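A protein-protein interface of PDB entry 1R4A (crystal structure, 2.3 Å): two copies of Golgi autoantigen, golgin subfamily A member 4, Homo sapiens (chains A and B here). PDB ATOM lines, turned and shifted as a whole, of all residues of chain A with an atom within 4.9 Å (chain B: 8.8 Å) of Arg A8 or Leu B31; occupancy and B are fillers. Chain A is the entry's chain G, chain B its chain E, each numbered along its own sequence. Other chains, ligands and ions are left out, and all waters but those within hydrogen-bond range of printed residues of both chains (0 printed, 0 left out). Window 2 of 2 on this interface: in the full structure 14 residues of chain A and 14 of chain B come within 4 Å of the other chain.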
ATOM      1  N   PHE A   4       1.237 -16.815  21.105  1.00  0.00           N
ATOM      2  CA  PHE A   4       1.626 -17.780  22.134  1.00  0.00           C
ATOM      3  C   PHE A   4       1.452 -19.188  21.600  1.00  0.00           C
ATOM      4  O   PHE A   4       2.378 -19.992  21.651  1.00  0.00           O
ATOM      5  CB  PHE A   4       0.778 -17.617  23.401  1.00  0.00           C
ATOM      6  CG  PHE A   4       1.507 -16.961  24.531  1.00  0.00           C
ATOM      7  CD1 PHE A   4       1.741 -15.591  24.517  1.00  0.00           C
ATOM      8  CD2 PHE A   4       1.994 -17.718  25.596  1.00  0.00           C
ATOM      9  CE1 PHE A   4       2.455 -14.970  25.553  1.00  0.00           C
ATOM     10  CE2 PHE A   4       2.709 -17.117  26.626  1.00  0.00           C
ATOM     11  CZ  PHE A   4       2.941 -15.740  26.605  1.00  0.00           C
ATOM     12  N   GLU A   5       0.256 -19.479  21.094  1.00  0.00           N
ATOM     13  CA  GLU A   5      -0.029 -20.797  20.532  1.00  0.00           C
ATOM     14  C   GLU A   5       1.020 -21.058  19.458  1.00  0.00           C
ATOM     15  O   GLU A   5       1.575 -22.154  19.365  1.00  0.00           O
ATOM     16  CB  GLU A   5      -1.432 -20.831  19.900  1.00  0.00           C
ATOM     17  CG  GLU A   5      -1.912 -22.240  19.549  1.00  0.00           C
ATOM     18  CD  GLU A   5      -3.240 -22.270  18.779  1.00  0.00           C
ATOM     19  OE1 GLU A   5      -4.119 -21.403  19.020  1.00  0.00           O
ATOM     20  OE2 GLU A   5      -3.410 -23.184  17.942  1.00  0.00           O
ATOM     21  N   TYR A   6       1.285 -20.031  18.652  1.00  0.00           N
ATOM     22  CA  TYR A   6       2.263 -20.143  17.580  1.00  0.00           C
ATOM     23  C   TYR A   6       3.600 -20.572  18.194  1.00  0.00           C
ATOM     24  O   TYR A   6       4.156 -21.599  17.817  1.00  0.00           O
ATOM     25  CB  TYR A   6       2.393 -18.796  16.853  1.00  0.00           C
ATOM     26  CG  TYR A   6       3.333 -18.819  15.665  1.00  0.00           C
ATOM     27  CD1 TYR A   6       2.947 -19.392  14.447  1.00  0.00           C
ATOM     28  CD2 TYR A   6       4.626 -18.302  15.770  1.00  0.00           C
ATOM     29  CE1 TYR A   6       3.837 -19.454  13.364  1.00  0.00           C
ATOM     30  CE2 TYR A   6       5.520 -18.355  14.700  1.00  0.00           C
ATOM     31  CZ  TYR A   6       5.123 -18.936  13.502  1.00  0.00           C
ATOM     32  OH  TYR A   6       6.030 -19.041  12.478  1.00  0.00           O
ATOM     33  N   LEU A   7       4.093 -19.786  19.148  1.00  0.00           N
ATOM     34  CA  LEU A   7       5.345 -20.078  19.849  1.00  0.00           C
ATOM     35  C   LEU A   7       5.349 -21.498  20.419  1.00  0.00           C
ATOM     36  O   LEU A   7       6.325 -22.239  20.271  1.00  0.00           O
ATOM     37  CB  LEU A   7       5.561 -19.089  20.999  1.00  0.00           C
ATOM     38  CG  LEU A   7       6.830 -19.329  21.825  1.00  0.00           C
ATOM     39  CD1 LEU A   7       8.065 -19.142  20.956  1.00  0.00           C
ATOM     40  CD2 LEU A   7       6.865 -18.375  22.988  1.00  0.00           C
ATOM     41  N   ARG A   8       4.261 -21.865  21.089  1.00  0.00           N
ATOM     42  CA  ARG A   8       4.146 -23.199  21.660  1.00  0.00           C
ATOM     43  C   ARG A   8       4.261 -24.255  20.566  1.00  0.00           C
ATOM     44  O   ARG A   8       4.915 -25.279  20.752  1.00  0.00           O
ATOM     45  CB  ARG A   8       2.810 -23.347  22.405  1.00  0.00           C
ATOM     46  CG  ARG A   8       2.879 -22.985  23.892  1.00  0.00           C
ATOM     47  CD  ARG A   8       1.505 -22.618  24.467  1.00  0.00           C
ATOM     48  NE  ARG A   8       0.461 -23.560  24.059  1.00  0.00           N
ATOM     49  CZ  ARG A   8      -0.753 -23.198  23.643  1.00  0.00           C
ATOM     50  NH1 ARG A   8      -1.637 -24.123  23.286  1.00  0.00           N
ATOM     51  NH2 ARG A   8      -1.085 -21.910  23.583  1.00  0.00           N
ATOM     52  N   LYS A   9       3.634 -23.995  19.422  1.00  0.00           N
ATOM     53  CA  LYS A   9       3.666 -24.922  18.294  1.00  0.00           C
ATOM     54  C   LYS A   9       5.091 -25.129  17.784  1.00  0.00           C
ATOM     55  O   LYS A   9       5.550 -26.255  17.639  1.00  0.00           O
ATOM     56  CB  LYS A   9       2.791 -24.383  17.153  1.00  0.00           C
ATOM     57  CG  LYS A   9       2.163 -25.459  16.263  1.00  0.00           C
ATOM     58  CD  LYS A   9       3.193 -26.238  15.459  1.00  0.00           C
ATOM     59  CE  LYS A   9       2.523 -27.347  14.648  1.00  0.00           C
ATOM     60  NZ  LYS A   9       3.476 -28.103  13.785  1.00  0.00           N
ATOM     61  N   VAL A  10       5.778 -24.025  17.502  1.00  0.00           N
ATOM     62  CA  VAL A  10       7.146 -24.068  16.996  1.00  0.00           C
ATOM     63  C   VAL A  10       8.155 -24.629  18.018  1.00  0.00           C
ATOM     64  O   VAL A  10       9.188 -25.192  17.641  1.00  0.00           O
ATOM     65  CB  VAL A  10       7.601 -22.647  16.541  1.00  0.00           C
ATOM     66  CG1 VAL A  10       9.078 -22.653  16.225  1.00  0.00           C
ATOM     67  CG2 VAL A  10       6.818 -22.218  15.285  1.00  0.00           C
ATOM     68  N   LEU A  11       7.853 -24.467  19.305  1.00  0.00           N
ATOM     69  CA  LEU A  11       8.729 -24.963  20.356  1.00  0.00           C
ATOM     70  C   LEU A  11       8.631 -26.489  20.424  1.00  0.00           C
ATOM     71  O   LEU A  11       9.640 -27.181  20.526  1.00  0.00           O
ATOM     72  CB  LEU A  11       8.342 -24.339  21.700  1.00  0.00           C
ATOM     73  CG  LEU A  11       9.489 -23.872  22.609  1.00  0.00           C
ATOM     74  CD1 LEU A  11      10.786 -23.749  21.839  1.00  0.00           C
ATOM     75  CD2 LEU A  11       9.115 -22.520  23.214  1.00  0.00           C
ATOM     76  N   PHE A  12       7.407 -26.997  20.334  1.00  0.00           N
ATOM     77  CA  PHE A  12       7.160 -28.432  20.361  1.00  0.00           C
ATOM     78  C   PHE A  12       7.935 -29.145  19.262  1.00  0.00           C
ATOM     79  O   PHE A  12       8.648 -30.119  19.513  1.00  0.00           O
ATOM     80  CB  PHE A  12       5.680 -28.718  20.165  1.00  0.00           C
ATOM     81  CG  PHE A  12       5.350 -30.180  20.184  1.00  0.00           C
ATOM     82  CD1 PHE A  12       5.397 -30.902  21.380  1.00  0.00           C
ATOM     83  CD2 PHE A  12       5.034 -30.854  19.004  1.00  0.00           C
ATOM     84  CE1 PHE A  12       5.136 -32.271  21.393  1.00  0.00           C
ATOM     85  CE2 PHE A  12       4.776 -32.223  19.011  1.00  0.00           C
ATOM     86  CZ  PHE A  12       4.826 -32.933  20.202  1.00  0.00           C
ATOM     87  N   GLU B   3       8.878 -13.187  33.467  1.00  0.00           N
ATOM     88  CA  GLU B   3       8.887 -14.578  33.063  1.00  0.00           C
ATOM     89  C   GLU B   3       9.394 -14.698  31.624  1.00  0.00           C
ATOM     90  O   GLU B   3       9.941 -15.730  31.235  1.00  0.00           O
ATOM     91  CB  GLU B   3       7.489 -15.172  33.193  1.00  0.00           C
ATOM     92  CG  GLU B   3       6.925 -15.028  34.590  1.00  0.00           C
ATOM     93  CD  GLU B   3       5.723 -15.908  34.824  1.00  0.00           C
ATOM     94  OE1 GLU B   3       5.874 -17.139  34.699  1.00  0.00           O
ATOM     95  OE2 GLU B   3       4.634 -15.379  35.132  1.00  0.00           O
ATOM     96  N   PHE B   4       9.232 -13.638  30.839  1.00  0.00           N
ATOM     97  CA  PHE B   4       9.695 -13.667  29.465  1.00  0.00           C
ATOM     98  C   PHE B   4      11.209 -13.662  29.388  1.00  0.00           C
ATOM     99  O   PHE B   4      11.791 -14.418  28.620  1.00  0.00           O
ATOM    100  CB  PHE B   4       9.120 -12.505  28.660  1.00  0.00           C
ATOM    101  CG  PHE B   4       7.818 -12.832  27.990  1.00  0.00           C
ATOM    102  CD1 PHE B   4       6.605 -12.617  28.641  1.00  0.00           C
ATOM    103  CD2 PHE B   4       7.811 -13.409  26.730  1.00  0.00           C
ATOM    104  CE1 PHE B   4       5.397 -12.978  28.040  1.00  0.00           C
ATOM    105  CE2 PHE B   4       6.615 -13.773  26.121  1.00  0.00           C
ATOM    106  CZ  PHE B   4       5.403 -13.557  26.774  1.00  0.00           C
ATOM    107  N   TYR B   6      12.970 -14.648  31.668  1.00  0.00           N
ATOM    108  CA  TYR B   6      13.259 -15.925  32.305  1.00  0.00           C
ATOM    109  C   TYR B   6      13.260 -17.009  31.236  1.00  0.00           C
ATOM    110  O   TYR B   6      14.263 -17.705  31.047  1.00  0.00           O
ATOM    111  CB  TYR B   6      12.197 -16.235  33.369  1.00  0.00           C
ATOM    112  CG  TYR B   6      12.478 -17.480  34.193  1.00  0.00           C
ATOM    113  CD1 TYR B   6      13.493 -17.497  35.145  1.00  0.00           C
ATOM    114  CD2 TYR B   6      11.740 -18.650  33.998  1.00  0.00           C
ATOM    115  CE1 TYR B   6      13.777 -18.651  35.884  1.00  0.00           C
ATOM    116  CE2 TYR B   6      12.011 -19.807  34.728  1.00  0.00           C
ATOM    117  CZ  TYR B   6      13.033 -19.803  35.664  1.00  0.00           C
ATOM    118  OH  TYR B   6      13.353 -20.962  36.334  1.00  0.00           O
ATOM    119  N   LEU B   7      12.138 -17.129  30.526  1.00  0.00           N
ATOM    120  CA  LEU B   7      11.975 -18.134  29.472  1.00  0.00           C
ATOM    121  C   LEU B   7      13.102 -18.060  28.459  1.00  0.00           C
ATOM    122  O   LEU B   7      13.651 -19.078  28.051  1.00  0.00           O
ATOM    123  CB  LEU B   7      10.622 -17.965  28.763  1.00  0.00           C
ATOM    124  CG  LEU B   7      10.305 -18.960  27.641  1.00  0.00           C
ATOM    125  CD1 LEU B   7      10.371 -20.378  28.151  1.00  0.00           C
ATOM    126  CD2 LEU B   7       8.924 -18.682  27.087  1.00  0.00           C
ATOM    127  N   ARG B   8      13.454 -16.842  28.082  1.00  0.00           N
ATOM    128  CA  ARG B   8      14.517 -16.642  27.118  1.00  0.00           C
ATOM    129  C   ARG B   8      15.838 -17.135  27.656  1.00  0.00           C
ATOM    130  O   ARG B   8      16.626 -17.756  26.936  1.00  0.00           O
ATOM    131  CB  ARG B   8      14.602 -15.165  26.741  1.00  0.00           C
ATOM    132  CG  ARG B   8      13.833 -14.853  25.453  1.00  0.00           C
ATOM    133  CD  ARG B   8      13.372 -13.409  25.393  1.00  0.00           C
ATOM    134  NE  ARG B   8      14.418 -12.488  25.817  1.00  0.00           N
ATOM    135  CZ  ARG B   8      14.173 -11.348  26.451  1.00  0.00           C
ATOM    136  NH1 ARG B   8      15.181 -10.560  26.813  1.00  0.00           N
ATOM    137  NH2 ARG B   8      12.918 -11.003  26.732  1.00  0.00           N
ATOM    138  N   LEU B  11      15.597 -21.012  27.665  1.00  0.00           N
ATOM    139  CA  LEU B  11      15.567 -21.521  26.287  1.00  0.00           C
ATOM    140  C   LEU B  11      16.979 -21.480  25.692  1.00  0.00           C
ATOM    141  O   LEU B  11      17.424 -22.426  25.035  1.00  0.00           O
ATOM    142  CB  LEU B  11      14.607 -20.654  25.460  1.00  0.00           C
ATOM    143  CG  LEU B  11      13.449 -21.223  24.630  1.00  0.00           C
ATOM    144  CD1 LEU B  11      13.127 -22.661  24.968  1.00  0.00           C
ATOM    145  CD2 LEU B  11      12.249 -20.332  24.860  1.00  0.00           C
ATOM    146  N   ALA B  24      14.267 -28.660  29.875  1.00  0.00           N
ATOM    147  CA  ALA B  24      13.051 -29.208  29.282  1.00  0.00           C
ATOM    148  C   ALA B  24      11.913 -29.178  30.280  1.00  0.00           C
ATOM    149  O   ALA B  24      10.773 -28.849  29.943  1.00  0.00           O
ATOM    150  CB  ALA B  24      13.294 -30.638  28.824  1.00  0.00           C
ATOM    151  N   LYS B  25      12.228 -29.513  31.532  1.00  0.00           N
ATOM    152  CA  LYS B  25      11.206 -29.497  32.567  1.00  0.00           C
ATOM    153  C   LYS B  25      10.669 -28.088  32.826  1.00  0.00           C
ATOM    154  O   LYS B  25       9.455 -27.892  32.926  1.00  0.00           O
ATOM    155  CB  LYS B  25      11.759 -30.104  33.864  1.00  0.00           C
ATOM    156  CG  LYS B  25      12.175 -31.578  33.736  1.00  0.00           C
ATOM    157  CD  LYS B  25      12.690 -32.132  35.056  1.00  0.00           C
ATOM    158  CE  LYS B  25      11.616 -32.072  36.143  1.00  0.00           C
ATOM    159  NZ  LYS B  25      12.104 -32.625  37.445  1.00  0.00           N
ATOM    160  N   VAL B  26      11.540 -27.092  32.922  1.00  0.00           N
ATOM    161  CA  VAL B  26      11.033 -25.744  33.186  1.00  0.00           C
ATOM    162  C   VAL B  26      10.321 -25.109  31.978  1.00  0.00           C
ATOM    163  O   VAL B  26       9.315 -24.402  32.139  1.00  0.00           O
ATOM    164  CB  VAL B  26      12.154 -24.791  33.736  1.00  0.00           C
ATOM    165  CG1 VAL B  26      13.499 -25.437  33.605  1.00  0.00           C
ATOM    166  CG2 VAL B  26      12.129 -23.448  33.008  1.00  0.00           C
ATOM    167  N   ILE B  27      10.805 -25.370  30.767  1.00  0.00           N
ATOM    168  CA  ILE B  27      10.164 -24.804  29.576  1.00  0.00           C
ATOM    169  C   ILE B  27       8.712 -25.279  29.469  1.00  0.00           C
ATOM    170  O   ILE B  27       7.795 -24.467  29.318  1.00  0.00           O
ATOM    171  CB  ILE B  27      10.925 -25.197  28.290  1.00  0.00           C
ATOM    172  CG1 ILE B  27      12.266 -24.470  28.247  1.00  0.00           C
ATOM    173  CG2 ILE B  27      10.080 -24.843  27.048  1.00  0.00           C
ATOM    174  CD1 ILE B  27      13.251 -25.045  27.260  1.00  0.00           C
ATOM    175  N   THR B  28       8.510 -26.592  29.572  1.00  0.00           N
ATOM    176  CA  THR B  28       7.174 -27.163  29.464  1.00  0.00           C
ATOM    177  C   THR B  28       6.241 -26.777  30.598  1.00  0.00           C
ATOM    178  O   THR B  28       5.022 -26.831  30.441  1.00  0.00           O
ATOM    179  CB  THR B  28       7.228 -28.697  29.358  1.00  0.00           C
ATOM    180  OG1 THR B  28       8.037 -29.225  30.419  1.00  0.00           O
ATOM    181  CG2 THR B  28       7.822 -29.112  28.012  1.00  0.00           C
ATOM    182  N   THR B  29       6.811 -26.381  31.739  1.00  0.00           N
ATOM    183  CA  THR B  29       5.998 -25.967  32.883  1.00  0.00           C
ATOM    184  C   THR B  29       5.615 -24.499  32.735  1.00  0.00           C
ATOM    185  O   THR B  29       4.474 -24.105  33.000  1.00  0.00           O
ATOM    186  CB  THR B  29       6.768 -26.168  34.227  1.00  0.00           C
ATOM    187  OG1 THR B  29       6.994 -27.564  34.450  1.00  0.00           O
ATOM    188  CG2 THR B  29       5.976 -25.607  35.394  1.00  0.00           C
ATOM    189  N   VAL B  30       6.574 -23.681  32.317  1.00  0.00           N
ATOM    190  CA  VAL B  30       6.323 -22.254  32.138  1.00  0.00           C
ATOM    191  C   VAL B  30       5.273 -22.005  31.050  1.00  0.00           C
ATOM    192  O   VAL B  30       4.359 -21.199  31.240  1.00  0.00           O
ATOM    193  CB  VAL B  30       7.628 -21.503  31.766  1.00  0.00           C
ATOM    194  CG1 VAL B  30       7.324 -20.045  31.464  1.00  0.00           C
ATOM    195  CG2 VAL B  30       8.634 -21.608  32.914  1.00  0.00           C
ATOM    196  N   LEU B  31       5.395 -22.695  29.915  1.00  0.00           N
ATOM    197  CA  LEU B  31       4.449 -22.539  28.806  1.00  0.00           C
ATOM    198  C   LEU B  31       3.228 -23.461  28.915  1.00  0.00           C
ATOM    199  O   LEU B  31       2.452 -23.591  27.964  1.00  0.00           O
ATOM    200  CB  LEU B  31       5.158 -22.761  27.464  1.00  0.00           C
ATOM    201  CG  LEU B  31       6.226 -21.718  27.118  1.00  0.00           C
ATOM    202  CD1 LEU B  31       6.835 -22.045  25.769  1.00  0.00           C
ATOM    203  CD2 LEU B  31       5.611 -20.324  27.099  1.00  0.00           C
ATOM    204  N   LYS B  32       3.072 -24.101  30.073  1.00  0.00           N
ATOM    205  CA  LYS B  32       1.932 -24.975  30.339  1.00  0.00           C
ATOM    206  C   LYS B  32       1.550 -25.983  29.237  1.00  0.00           C
ATOM    207  O   LYS B  32       0.392 -26.040  28.817  1.00  0.00           O
ATOM    208  CB  LYS B  32       0.709 -24.111  30.663  1.00  0.00           C
ATOM    209  CG  LYS B  32       0.961 -23.041  31.721  1.00  0.00           C
ATOM    210  CD  LYS B  32      -0.119 -21.964  31.660  1.00  0.00           C
ATOM    211  CE  LYS B  32       0.076 -20.881  32.718  1.00  0.00           C
ATOM    212  NZ  LYS B  32      -0.212 -21.373  34.099  1.00  0.00           N
ATOM    213  N   PHE B  33       2.508 -26.781  28.777  1.00  0.00           N
ATOM    214  CA  PHE B  33       2.229 -27.779  27.747  1.00  0.00           C
ATOM    215  C   PHE B  33       1.311 -28.868  28.313  1.00  0.00           C
ATOM    216  O   PHE B  33       1.277 -29.092  29.521  1.00  0.00           O
ATOM    217  CB  PHE B  33       3.523 -28.447  27.281  1.00  0.00           C
ATOM    218  CG  PHE B  33       4.323 -27.633  26.303  1.00  0.00           C
ATOM    219  CD1 PHE B  33       4.585 -26.289  26.534  1.00  0.00           C
ATOM    220  CD2 PHE B  33       4.862 -28.228  25.170  1.00  0.00           C
ATOM    221  CE1 PHE B  33       5.375 -25.559  25.655  1.00  0.00           C
ATOM    222  CE2 PHE B  33       5.654 -27.503  24.288  1.00  0.00           C
ATOM    223  CZ  PHE B  33       5.909 -26.167  24.533  1.00  0.00           C
ATOM    224  N   PRO B  34       0.557 -29.564  27.442  1.00  0.00           N
ATOM    225  CA  PRO B  34      -0.350 -30.634  27.878  1.00  0.00           C
ATOM    226  C   PRO B  34       0.436 -31.879  28.302  1.00  0.00           C
ATOM    227  O   PRO B  34       1.498 -32.172  27.741  1.00  0.00           O
ATOM    228  CB  PRO B  34      -1.202 -30.877  26.647  1.00  0.00           C
ATOM    229  CG  PRO B  34      -0.226 -30.626  25.541  1.00  0.00           C
ATOM    230  CD  PRO B  34       0.459 -29.361  25.994  1.00  0.00           C
ATOM    231  N   GLN B  37       2.122 -34.225  25.399  1.00  0.00           N
ATOM    232  CA  GLN B  37       3.287 -33.641  24.736  1.00  0.00           C
ATOM    233  C   GLN B  37       4.486 -33.478  25.668  1.00  0.00           C
ATOM    234  O   GLN B  37       5.634 -33.660  25.259  1.00  0.00           O
ATOM    235  CB  GLN B  37       2.926 -32.281  24.127  1.00  0.00           C
ATOM    236  CG  GLN B  37       2.014 -32.362  22.910  1.00  0.00           C
ATOM    237  CD  GLN B  37       1.734 -31.001  22.290  1.00  0.00           C
ATOM    238  OE1 GLN B  37       1.175 -30.113  22.934  1.00  0.00           O
ATOM    239  NE2 GLN B  37       2.126 -30.831  21.031  1.00  0.00           N
ATOM    240  N   THR B  38       4.220 -33.126  26.919  1.00  0.00           N
ATOM    241  CA  THR B  38       5.292 -32.959  27.880  1.00  0.00           C
ATOM    242  C   THR B  38       5.966 -34.313  28.119  1.00  0.00           C
ATOM    243  O   THR B  38       7.187 -34.385  28.241  1.00  0.00           O
ATOM    244  CB  THR B  38       4.773 -32.431  29.215  1.00  0.00           C
ATOM    245  OG1 THR B  38       4.189 -31.139  29.030  1.00  0.00           O
ATOM    246  CG2 THR B  38       5.908 -32.330  30.215  1.00  0.00           C
ATOM    247  N   ILE B  41       8.085 -35.341  25.173  1.00  0.00           N
ATOM    248  CA  ILE B  41       9.339 -34.594  25.201  1.00  0.00           C
ATOM    249  C   ILE B  41      10.299 -35.179  26.246  1.00  0.00           C
ATOM    250  O   ILE B  41      11.458 -35.454  25.942  1.00  0.00           O
ATOM    251  CB  ILE B  41       9.075 -33.101  25.531  1.00  0.00           C
ATOM    252  CG1 ILE B  41       8.257 -32.454  24.412  1.00  0.00           C
ATOM    253  CG2 ILE B  41      10.389 -32.359  25.739  1.00  0.00           C
ATOM    254  CD1 ILE B  41       7.887 -31.003  24.669  1.00  0.00           C
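O of Thr B28 sits at hydrogen-bond distance from N of Phe B33 (3.0 Å).
Printed residues of chain B within 4 Å of Arg A8: Leu B31 (3.8 Å) and Phe B33 (3.995 Å).
Of the printed residues of chain A, Gln B37 touches Phe A12 (3.3 Å).
Printed residues of chain B within 4 Å of Phe A4: Phe B4 (3.3 Å).
Printed residues of chain B within 4 Å of Leu A11: Leu B31.
Of the printed residues of chain A, Phe B4 touches Phe A4.
Of the printed residues of chain A, Phe B33 touches Arg A8 (3.995 Å).
The nearest printed residue of chain B that does not touch Arg A8 is Lys B32 (5.4 Å).
The nearest residue of chain A that does not touch Leu B31 is Phe A4 (4.4 Å).
Of the 20 printed residues of chain B, 4 touch a printed residue of chain A.
Among the printed residues, no Asp or Glu carboxylate lies within 4 Å of a Lys or Arg side-chain nitrogen of the other chain.
Phe B4 touches its own counterpart, Phe A4.
Positions printed for both chains: 4, 6, 7, 8 and 11.
Among the printed residues, pairs that only touch across the chains: Phe A12 with Gln B37, Phe A4 with Phe B4, Leu A11 with Leu B31, Arg A8 with Leu B31 and Arg A8 with Phe B33.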
